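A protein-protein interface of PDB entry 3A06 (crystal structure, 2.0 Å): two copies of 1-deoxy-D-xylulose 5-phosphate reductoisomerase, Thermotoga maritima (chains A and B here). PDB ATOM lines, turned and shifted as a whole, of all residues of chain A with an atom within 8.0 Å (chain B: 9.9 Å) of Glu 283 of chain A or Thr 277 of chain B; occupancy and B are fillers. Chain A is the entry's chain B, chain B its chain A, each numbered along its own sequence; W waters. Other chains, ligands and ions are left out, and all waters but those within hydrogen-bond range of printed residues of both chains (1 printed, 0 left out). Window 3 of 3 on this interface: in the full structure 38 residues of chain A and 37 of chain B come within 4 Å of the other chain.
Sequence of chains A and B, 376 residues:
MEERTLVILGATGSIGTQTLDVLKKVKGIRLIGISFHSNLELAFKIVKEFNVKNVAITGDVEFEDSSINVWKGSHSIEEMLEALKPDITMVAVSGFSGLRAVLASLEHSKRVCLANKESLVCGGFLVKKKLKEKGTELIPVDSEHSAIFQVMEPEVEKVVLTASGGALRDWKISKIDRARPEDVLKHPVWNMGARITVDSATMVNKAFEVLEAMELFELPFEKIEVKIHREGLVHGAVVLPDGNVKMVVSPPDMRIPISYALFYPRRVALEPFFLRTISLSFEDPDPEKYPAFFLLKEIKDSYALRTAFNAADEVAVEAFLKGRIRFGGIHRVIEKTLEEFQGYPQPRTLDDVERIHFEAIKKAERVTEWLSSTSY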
ATOM      1  N   LEU A 161      36.068  11.454  -1.557  1.00  0.00           N
ATOM      2  CA  LEU A 161      36.178  12.924  -1.598  1.00  0.00           C
ATOM      3  C   LEU A 161      35.491  13.361  -2.859  1.00  0.00           C
ATOM      4  O   LEU A 161      35.618  12.709  -3.891  1.00  0.00           O
ATOM      5  CB  LEU A 161      37.654  13.378  -1.650  1.00  0.00           C
ATOM      6  CG  LEU A 161      38.609  12.797  -0.589  1.00  0.00           C
ATOM      7  CD1 LEU A 161      40.060  13.285  -0.786  1.00  0.00           C
ATOM      8  CD2 LEU A 161      38.123  13.181   0.791  1.00  0.00           C
ATOM      9  N   THR A 162      34.764  14.459  -2.805  1.00  0.00           N
ATOM     10  CA  THR A 162      34.091  14.916  -4.020  1.00  0.00           C
ATOM     11  C   THR A 162      34.829  16.116  -4.559  1.00  0.00           C
ATOM     12  O   THR A 162      35.464  16.868  -3.787  1.00  0.00           O
ATOM     13  CB  THR A 162      32.642  15.315  -3.742  1.00  0.00           C
ATOM     14  OG1 THR A 162      32.647  16.238  -2.650  1.00  0.00           O
ATOM     15  CG2 THR A 162      31.825  14.085  -3.345  1.00  0.00           C
ATOM     16  N   ALA A 163      34.741  16.281  -5.873  1.00  0.00           N
ATOM     17  CA  ALA A 163      35.404  17.374  -6.590  1.00  0.00           C
ATOM     18  C   ALA A 163      34.382  18.004  -7.505  1.00  0.00           C
ATOM     19  O   ALA A 163      33.604  17.300  -8.158  1.00  0.00           O
ATOM     20  CB  ALA A 163      36.560  16.825  -7.437  1.00  0.00           C
ATOM     21  N   MET A 203      42.582  19.711 -10.978  1.00  0.00           N
ATOM     22  CA  MET A 203      42.388  18.773  -9.863  1.00  0.00           C
ATOM     23  C   MET A 203      43.646  18.455  -9.041  1.00  0.00           C
ATOM     24  O   MET A 203      43.702  17.469  -8.314  1.00  0.00           O
ATOM     25  CB  MET A 203      41.652  17.505 -10.318  1.00  0.00           C
ATOM     26  CG  MET A 203      40.129  17.789 -10.411  1.00  0.00           C
ATOM     27  SD  MET A 203      39.217  16.291 -10.871  1.00  0.00           S
ATOM     28  CE  MET A 203      39.512  15.268  -9.435  1.00  0.00           C
ATOM     29  N   VAL A 226      38.112   9.426  -5.398  1.00  0.00           N
ATOM     30  CA  VAL A 226      37.624  10.773  -5.724  1.00  0.00           C
ATOM     31  C   VAL A 226      36.553  10.694  -6.804  1.00  0.00           C
ATOM     32  O   VAL A 226      36.727   9.995  -7.802  1.00  0.00           O
ATOM     33  CB  VAL A 226      38.763  11.737  -6.138  1.00  0.00           C
ATOM     34  CG1 VAL A 226      38.226  13.104  -6.573  1.00  0.00           C
ATOM     35  CG2 VAL A 226      39.724  11.934  -4.958  1.00  0.00           C
ATOM     36  N   LYS A 227      35.438  11.385  -6.578  1.00  0.00           N
ATOM     37  CA  LYS A 227      34.355  11.436  -7.540  1.00  0.00           C
ATOM     38  C   LYS A 227      34.090  12.860  -7.910  1.00  0.00           C
ATOM     39  O   LYS A 227      34.011  13.723  -7.052  1.00  0.00           O
ATOM     40  CB  LYS A 227      33.081  10.841  -6.920  1.00  0.00           C
ATOM     41  CG  LYS A 227      33.187   9.336  -6.573  1.00  0.00           C
ATOM     42  CD  LYS A 227      33.077   8.474  -7.837  1.00  0.00           C
ATOM     43  CE  LYS A 227      33.257   6.983  -7.514  1.00  0.00           C
ATOM     44  NZ  LYS A 227      33.191   6.166  -8.756  1.00  0.00           N
ATOM     45  N   ILE A 228      33.891  13.118  -9.194  1.00  0.00           N
ATOM     46  CA  ILE A 228      33.366  14.406  -9.601  1.00  0.00           C
ATOM     47  C   ILE A 228      31.869  14.481  -9.266  1.00  0.00           C
ATOM     48  O   ILE A 228      31.097  13.611  -9.622  1.00  0.00           O
ATOM     49  CB  ILE A 228      33.688  14.691 -11.067  1.00  0.00           C
ATOM     50  CG1 ILE A 228      35.183  15.097 -11.155  1.00  0.00           C
ATOM     51  CG2 ILE A 228      32.854  15.817 -11.593  1.00  0.00           C
ATOM     52  CD1 ILE A 228      35.684  15.134 -12.531  1.00  0.00           C
ATOM     53  N   HIS A 229      31.486  15.539  -8.574  1.00  0.00           N
ATOM     54  CA  HIS A 229      30.148  15.671  -8.045  1.00  0.00           C
ATOM     55  C   HIS A 229      29.660  17.050  -8.426  1.00  0.00           C
ATOM     56  O   HIS A 229      29.919  18.015  -7.710  1.00  0.00           O
ATOM     57  CB  HIS A 229      30.194  15.501  -6.527  1.00  0.00           C
ATOM     58  CG  HIS A 229      28.905  15.815  -5.846  1.00  0.00           C
ATOM     59  ND1 HIS A 229      27.701  15.268  -6.239  1.00  0.00           N
ATOM     60  CD2 HIS A 229      28.621  16.663  -4.833  1.00  0.00           C
ATOM     61  CE1 HIS A 229      26.738  15.731  -5.460  1.00  0.00           C
ATOM     62  NE2 HIS A 229      27.269  16.582  -4.602  1.00  0.00           N
ATOM     63  N   ARG A 230      28.975  17.160  -9.559  1.00  0.00           N
ATOM     64  CA  ARG A 230      28.730  18.498 -10.121  1.00  0.00           C
ATOM     65  C   ARG A 230      27.826  19.435  -9.282  1.00  0.00           C
ATOM     66  O   ARG A 230      27.921  20.665  -9.410  1.00  0.00           O
ATOM     67  CB  ARG A 230      28.344  18.445 -11.604  1.00  0.00           C
ATOM     68  CG  ARG A 230      26.888  18.226 -11.908  1.00  0.00           C
ATOM     69  CD  ARG A 230      26.641  18.194 -13.424  1.00  0.00           C
ATOM     70  NE  ARG A 230      26.655  19.530 -14.028  1.00  0.00           N
ATOM     71  CZ  ARG A 230      27.515  19.939 -14.970  1.00  0.00           C
ATOM     72  NH1 ARG A 230      27.428  21.173 -15.438  1.00  0.00           N
ATOM     73  NH2 ARG A 230      28.464  19.129 -15.445  1.00  0.00           N
ATOM     74  N   GLU A 231      26.977  18.881  -8.415  1.00  0.00           N
ATOM     75  CA  GLU A 231      26.162  19.738  -7.531  1.00  0.00           C
ATOM     76  C   GLU A 231      26.944  20.397  -6.387  1.00  0.00           C
ATOM     77  O   GLU A 231      26.521  21.421  -5.860  1.00  0.00           O
ATOM     78  CB  GLU A 231      24.944  18.981  -6.982  1.00  0.00           C
ATOM     79  CG  GLU A 231      23.988  18.474  -8.044  1.00  0.00           C
ATOM     80  CD  GLU A 231      24.485  17.237  -8.765  1.00  0.00           C
ATOM     81  OE1 GLU A 231      25.468  16.602  -8.319  1.00  0.00           O
ATOM     82  OE2 GLU A 231      23.875  16.878  -9.784  1.00  0.00           O
ATOM     83  N   SER A 279      18.975  15.413  -7.712  1.00  0.00           N
ATOM     84  CA  SER A 279      19.848  14.401  -8.263  1.00  0.00           C
ATOM     85  C   SER A 279      21.232  14.643  -7.645  1.00  0.00           C
ATOM     86  O   SER A 279      21.584  15.780  -7.299  1.00  0.00           O
ATOM     87  CB  SER A 279      19.888  14.475  -9.792  1.00  0.00           C
ATOM     88  OG  SER A 279      20.202  13.205 -10.349  1.00  0.00           O
ATOM     89  N   LEU A 280      21.983  13.569  -7.446  1.00  0.00           N
ATOM     90  CA  LEU A 280      23.345  13.686  -6.959  1.00  0.00           C
ATOM     91  C   LEU A 280      24.201  12.888  -7.908  1.00  0.00           C
ATOM     92  O   LEU A 280      23.960  11.705  -8.101  1.00  0.00           O
ATOM     93  CB  LEU A 280      23.483  13.169  -5.517  1.00  0.00           C
ATOM     94  CG  LEU A 280      22.703  13.859  -4.397  1.00  0.00           C
ATOM     95  CD1 LEU A 280      22.925  13.111  -3.092  1.00  0.00           C
ATOM     96  CD2 LEU A 280      23.051  15.326  -4.232  1.00  0.00           C
ATOM     97  N   SER A 281      25.176  13.553  -8.526  1.00  0.00           N
ATOM     98  CA  SER A 281      25.997  12.937  -9.550  1.00  0.00           C
ATOM     99  C   SER A 281      27.344  12.574  -8.965  1.00  0.00           C
ATOM    100  O   SER A 281      27.906  13.349  -8.203  1.00  0.00           O
ATOM    101  CB  SER A 281      26.194  13.902 -10.736  1.00  0.00           C
ATOM    102  OG  SER A 281      24.973  14.512 -11.119  1.00  0.00           O
ATOM    103  N   PHE A 282      27.837  11.391  -9.318  1.00  0.00           N
ATOM    104  CA  PHE A 282      29.180  10.932  -8.955  1.00  0.00           C
ATOM    105  C   PHE A 282      29.808  10.247 -10.171  1.00  0.00           C
ATOM    106  O   PHE A 282      29.331   9.191 -10.618  1.00  0.00           O
ATOM    107  CB  PHE A 282      29.130   9.978  -7.750  1.00  0.00           C
ATOM    108  CG  PHE A 282      28.470  10.570  -6.539  1.00  0.00           C
ATOM    109  CD1 PHE A 282      27.137  10.300  -6.261  1.00  0.00           C
ATOM    110  CD2 PHE A 282      29.179  11.410  -5.684  1.00  0.00           C
ATOM    111  CE1 PHE A 282      26.501  10.844  -5.147  1.00  0.00           C
ATOM    112  CE2 PHE A 282      28.562  11.973  -4.566  1.00  0.00           C
ATOM    113  CZ  PHE A 282      27.200  11.682  -4.296  1.00  0.00           C
ATOM    114  N   GLU A 283      30.852  10.850 -10.732  1.00  0.00           N
ATOM    115  CA  GLU A 283      31.508  10.272 -11.902  1.00  0.00           C
ATOM    116  C   GLU A 283      32.989  10.154 -11.603  1.00  0.00           C
ATOM    117  O   GLU A 283      33.507  10.927 -10.821  1.00  0.00           O
ATOM    118  CB  GLU A 283      31.348  11.166 -13.139  1.00  0.00           C
ATOM    119  CG  GLU A 283      30.096  12.038 -13.220  1.00  0.00           C
ATOM    120  CD  GLU A 283      28.822  11.260 -13.555  1.00  0.00           C
ATOM    121  OE1 GLU A 283      28.899  10.030 -13.845  1.00  0.00           O
ATOM    122  OE2 GLU A 283      27.731  11.892 -13.523  1.00  0.00           O
ATOM    123  N   ASP A 284      33.662   9.203 -12.234  1.00  0.00           N
ATOM    124  CA  ASP A 284      35.108   9.113 -12.128  1.00  0.00           C
ATOM    125  C   ASP A 284      35.739  10.257 -12.935  1.00  0.00           C
ATOM    126  O   ASP A 284      35.227  10.616 -14.001  1.00  0.00           O
ATOM    127  CB  ASP A 284      35.597   7.765 -12.654  1.00  0.00           C
ATOM    128  CG  ASP A 284      35.141   6.589 -11.787  1.00  0.00           C
ATOM    129  OD1 ASP A 284      35.076   5.463 -12.332  1.00  0.00           O
ATOM    130  OD2 ASP A 284      34.852   6.776 -10.567  1.00  0.00           O
ATOM    131  N   PRO A 285      36.840  10.852 -12.430  1.00  0.00           N
ATOM    132  CA  PRO A 285      37.551  11.855 -13.252  1.00  0.00           C
ATOM    133  C   PRO A 285      38.247  11.222 -14.460  1.00  0.00           C
ATOM    134  O   PRO A 285      38.893  10.188 -14.332  1.00  0.00           O
ATOM    135  CB  PRO A 285      38.603  12.429 -12.288  1.00  0.00           C
ATOM    136  CG  PRO A 285      38.118  12.002 -10.896  1.00  0.00           C
ATOM    137  CD  PRO A 285      37.481  10.666 -11.118  1.00  0.00           C
ATOM    138  N   ASP A 286      38.106  11.859 -15.618  1.00  0.00           N
ATOM    139  CA  ASP A 286      38.765  11.440 -16.849  1.00  0.00           C
ATOM    140  C   ASP A 286      40.288  11.694 -16.757  1.00  0.00           C
ATOM    141  O   ASP A 286      40.714  12.833 -16.623  1.00  0.00           O
ATOM    142  CB  ASP A 286      38.120  12.216 -18.022  1.00  0.00           C
ATOM    143  CG  ASP A 286      38.558  11.714 -19.409  1.00  0.00           C
ATOM    144  OD1 ASP A 286      37.920  12.125 -20.408  1.00  0.00           O
ATOM    145  OD2 ASP A 286      39.529  10.938 -19.515  1.00  0.00           O
ATOM    146  N   GLU B 231      12.436   6.646  -3.533  1.00  0.00           N
ATOM    147  CA  GLU B 231      13.489   5.672  -3.864  1.00  0.00           C
ATOM    148  C   GLU B 231      13.996   4.773  -2.736  1.00  0.00           C
ATOM    149  O   GLU B 231      14.574   3.715  -2.993  1.00  0.00           O
ATOM    150  CB  GLU B 231      14.642   6.351  -4.610  1.00  0.00           C
ATOM    151  CG  GLU B 231      14.973   7.730  -4.121  1.00  0.00           C
ATOM    152  CD  GLU B 231      14.102   8.825  -4.713  1.00  0.00           C
ATOM    153  OE1 GLU B 231      13.527   9.600  -3.929  1.00  0.00           O
ATOM    154  OE2 GLU B 231      14.021   8.942  -5.951  1.00  0.00           O
ATOM    155  N   LEU B 233      16.390   5.052  -0.560  1.00  0.00           N
ATOM    156  CA  LEU B 233      17.856   4.999  -0.385  1.00  0.00           C
ATOM    157  C   LEU B 233      18.346   5.637   0.913  1.00  0.00           C
ATOM    158  O   LEU B 233      19.156   5.047   1.615  1.00  0.00           O
ATOM    159  CB  LEU B 233      18.553   5.669  -1.557  1.00  0.00           C
ATOM    160  CG  LEU B 233      18.367   4.971  -2.903  1.00  0.00           C
ATOM    161  CD1 LEU B 233      19.113   5.760  -3.920  1.00  0.00           C
ATOM    162  CD2 LEU B 233      18.881   3.541  -2.818  1.00  0.00           C
ATOM    163  N   PHE B 273      28.058  -0.477  -0.886  1.00  0.00           N
ATOM    164  CA  PHE B 273      27.097   0.190  -1.748  1.00  0.00           C
ATOM    165  C   PHE B 273      27.834   1.246  -2.525  1.00  0.00           C
ATOM    166  O   PHE B 273      28.223   2.272  -1.968  1.00  0.00           O
ATOM    167  CB  PHE B 273      25.998   0.857  -0.920  1.00  0.00           C
ATOM    168  CG  PHE B 273      24.753   1.231  -1.717  1.00  0.00           C
ATOM    169  CD1 PHE B 273      24.257   0.397  -2.719  1.00  0.00           C
ATOM    170  CD2 PHE B 273      24.051   2.394  -1.424  1.00  0.00           C
ATOM    171  CE1 PHE B 273      23.096   0.730  -3.435  1.00  0.00           C
ATOM    172  CE2 PHE B 273      22.889   2.739  -2.149  1.00  0.00           C
ATOM    173  CZ  PHE B 273      22.420   1.911  -3.148  1.00  0.00           C
ATOM    174  N   PHE B 274      28.025   1.030  -3.815  1.00  0.00           N
ATOM    175  CA  PHE B 274      28.904   1.963  -4.496  1.00  0.00           C
ATOM    176  C   PHE B 274      28.240   3.153  -5.109  1.00  0.00           C
ATOM    177  O   PHE B 274      27.230   3.027  -5.809  1.00  0.00           O
ATOM    178  CB  PHE B 274      29.983   1.286  -5.341  1.00  0.00           C
ATOM    179  CG  PHE B 274      31.218   0.960  -4.543  1.00  0.00           C
ATOM    180  CD1 PHE B 274      31.596  -0.362  -4.314  1.00  0.00           C
ATOM    181  CD2 PHE B 274      31.976   1.984  -3.964  1.00  0.00           C
ATOM    182  CE1 PHE B 274      32.733  -0.656  -3.555  1.00  0.00           C
ATOM    183  CE2 PHE B 274      33.115   1.697  -3.205  1.00  0.00           C
ATOM    184  CZ  PHE B 274      33.495   0.373  -3.002  1.00  0.00           C
ATOM    185  N   LEU B 275      28.804   4.315  -4.777  1.00  0.00           N
ATOM    186  CA  LEU B 275      28.271   5.622  -5.168  1.00  0.00           C
ATOM    187  C   LEU B 275      28.057   5.744  -6.671  1.00  0.00           C
ATOM    188  O   LEU B 275      28.954   5.446  -7.456  1.00  0.00           O
ATOM    189  CB  LEU B 275      29.215   6.739  -4.689  1.00  0.00           C
ATOM    190  CG  LEU B 275      28.783   7.531  -3.448  1.00  0.00           C
ATOM    191  CD1 LEU B 275      28.405   6.628  -2.286  1.00  0.00           C
ATOM    192  CD2 LEU B 275      29.856   8.510  -3.027  1.00  0.00           C
ATOM    193  N   ARG B 276      26.869   6.184  -7.061  1.00  0.00           N
ATOM    194  CA  ARG B 276      26.599   6.510  -8.455  1.00  0.00           C
ATOM    195  C   ARG B 276      25.535   7.603  -8.532  1.00  0.00           C
ATOM    196  O   ARG B 276      24.935   7.969  -7.510  1.00  0.00           O
ATOM    197  CB  ARG B 276      26.191   5.255  -9.247  1.00  0.00           C
ATOM    198  CG  ARG B 276      24.846   4.648  -8.874  1.00  0.00           C
ATOM    199  CD  ARG B 276      24.784   4.279  -7.401  1.00  0.00           C
ATOM    200  NE  ARG B 276      23.510   3.674  -7.059  1.00  0.00           N
ATOM    201  CZ  ARG B 276      23.356   2.416  -6.663  1.00  0.00           C
ATOM    202  NH1 ARG B 276      24.408   1.607  -6.532  1.00  0.00           N
ATOM    203  NH2 ARG B 276      22.137   1.973  -6.385  1.00  0.00           N
ATOM    204  N   THR B 277      25.307   8.127  -9.732  1.00  0.00           N
ATOM    205  CA  THR B 277      24.308   9.172  -9.922  1.00  0.00           C
ATOM    206  C   THR B 277      22.945   8.634  -9.501  1.00  0.00           C
ATOM    207  O   THR B 277      22.629   7.457  -9.709  1.00  0.00           O
ATOM    208  CB  THR B 277      24.370   9.771 -11.342  1.00  0.00           C
ATOM    209  OG1 THR B 277      25.651  10.397 -11.497  1.00  0.00           O
ATOM    210  CG2 THR B 277      23.277  10.817 -11.576  1.00  0.00           C
ATOM    211  N   ILE B 278      22.178   9.497  -8.843  1.00  0.00           N
ATOM    212  CA  ILE B 278      21.123   9.041  -7.949  1.00  0.00           C
ATOM    213  C   ILE B 278      20.064  10.120  -7.781  1.00  0.00           C
ATOM    214  O   ILE B 278      20.350  11.312  -7.922  1.00  0.00           O
ATOM    215  CB  ILE B 278      21.737   8.624  -6.573  1.00  0.00           C
ATOM    216  CG1 ILE B 278      21.102   7.342  -6.039  1.00  0.00           C
ATOM    217  CG2 ILE B 278      21.747   9.773  -5.559  1.00  0.00           C
ATOM    218  CD1 ILE B 278      21.518   6.102  -6.806  1.00  0.00           C
ATOM    219  N   SER B 279      18.844   9.686  -7.486  1.00  0.00           N
ATOM    220  CA  SER B 279      17.698  10.587  -7.401  1.00  0.00           C
ATOM    221  C   SER B 279      17.158  10.569  -5.986  1.00  0.00           C
ATOM    222  O   SER B 279      16.810   9.512  -5.466  1.00  0.00           O
ATOM    223  CB  SER B 279      16.616  10.151  -8.389  1.00  0.00           C
ATOM    224  OG  SER B 279      17.177   9.974  -9.679  1.00  0.00           O
ATOM    225  N   LEU B 280      17.112  11.730  -5.349  1.00  0.00           N
ATOM    226  CA  LEU B 280      16.662  11.792  -3.973  1.00  0.00           C
ATOM    227  C   LEU B 280      15.527  12.788  -3.830  1.00  0.00           C
ATOM    228  O   LEU B 280      15.747  13.995  -3.813  1.00  0.00           O
ATOM    229  CB  LEU B 280      17.822  12.127  -3.024  1.00  0.00           C
ATOM    230  CG  LEU B 280      19.022  11.166  -2.958  1.00  0.00           C
ATOM    231  CD1 LEU B 280      20.013  11.625  -1.914  1.00  0.00           C
ATOM    232  CD2 LEU B 280      18.611   9.721  -2.681  1.00  0.00           C
HETATM  233  O   HOH W   1      27.219   7.005 -11.692  1.00  0.00           O
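The side-chain hydroxyl (OG1) of Thr 277 of chain B is in hydrogen-bond range of the backbone NH (N) of Phe 282 of chain A (3.2 Å). OG1 of Thr 277 of chain B lies within hydrogen-bond range of OE2 of Glu 283 of chain A (3.3 Å). O of Ile 278 of chain B is in hydrogen-bond range of OG of Ser 279 of chain A, 3.1 Å away. The backbone NH (N) of Leu 280 of chain A sits at hydrogen-bond distance from the backbone carbonyl oxygen (O) of Ile 278 of chain B (2.8 Å).
O of Phe 274 of chain B lies close to NH1 of Arg 276 of chain B (3.2 Å). The backbone NH (N) of Ile 228 of chain A sits at hydrogen-bond distance from the backbone carbonyl oxygen (O) of Glu 283 of chain A. A ring nitrogen (ND1) of His 229 of chain A lies within hydrogen-bond range of the backbone carbonyl oxygen (O) of Ser 281 of chain A (2.8 Å). OG of Ser 281 of chain A lies within hydrogen-bond range of OE2 of Glu 231 of chain A, 2.9 Å away.
O of Leu 280 of chain A touches O of Arg 276 of chain B, at 3.9 Å. Thr 277 of chain B touches Leu 280 of chain A. Leu 280 of chain B touches Leu 280 of chain A. CA of Ser 281 of chain A touches OG1 of Thr 277 of chain B (3.2 Å). Phe 282 of chain A touches Leu 275 of chain B. Phe 282 of chain A touches Arg 276 of chain B (CD1 to O, 3.4 Å).
Of the printed residues of chain B, Glu 283 of chain A touches Thr 277. No residue of chain B comes within 4 Å of Lys 227 of chain A. Ile 228 of chain A touches none of the printed residues of chain B. Ser 281 of chain A touches one residue of chain B. No residue of chain B comes within 4 Å of Asp 284 of chain A. Printed residues of chain A within 4 Å of Leu 275 of chain B: Phe 282 (3.99 Å). Printed residues of chain A within 4 Å of Leu 280 of chain B: Leu 280. The nearest residue of chain B that does not touch Glu 283 of chain A is Arg 276 of chain B (6.5 Å). The nearest printed residue of chain B that does not touch Ser 279 of chain A is Thr 277 of chain B (4.1 Å).
Of the 10 printed residues of chain B, 5 touch a printed residue of chain A. Hydrophobic or aromatic side chains of chain B within 4 Å of the printed part of chain A: Leu 275, Ile 278 and Leu 280. Of the 18 printed residues of chain A, 5 touch a printed residue of chain B. Printed residues of chain A that touch a printed residue of chain B: Ser 279, Leu 280, Ser 281, Phe 282 and Glu 283. Hydrophobic or aromatic side chains of chain A that line the printed part of chain B: Leu 280 and Phe 282. Among the printed residues, 10 pairs touch across the chains. Among the printed residues, no Asp or Glu carboxylate lies within 4 Å of a Lys or Arg side-chain nitrogen of the other chain.
Leu 280 of chain B touches its own counterpart, Leu 280 of chain A. Of the 10 pairs that touch across the chains among the printed residues, 1 has its exchanged pair printed and touching as well.
Water W1 lies within hydrogen-bond range of the backbone NH (N) of Thr 277 of chain B (3.0 Å) and the backbone carbonyl oxygen (O) of Phe 282 of chain A (3.2 Å).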
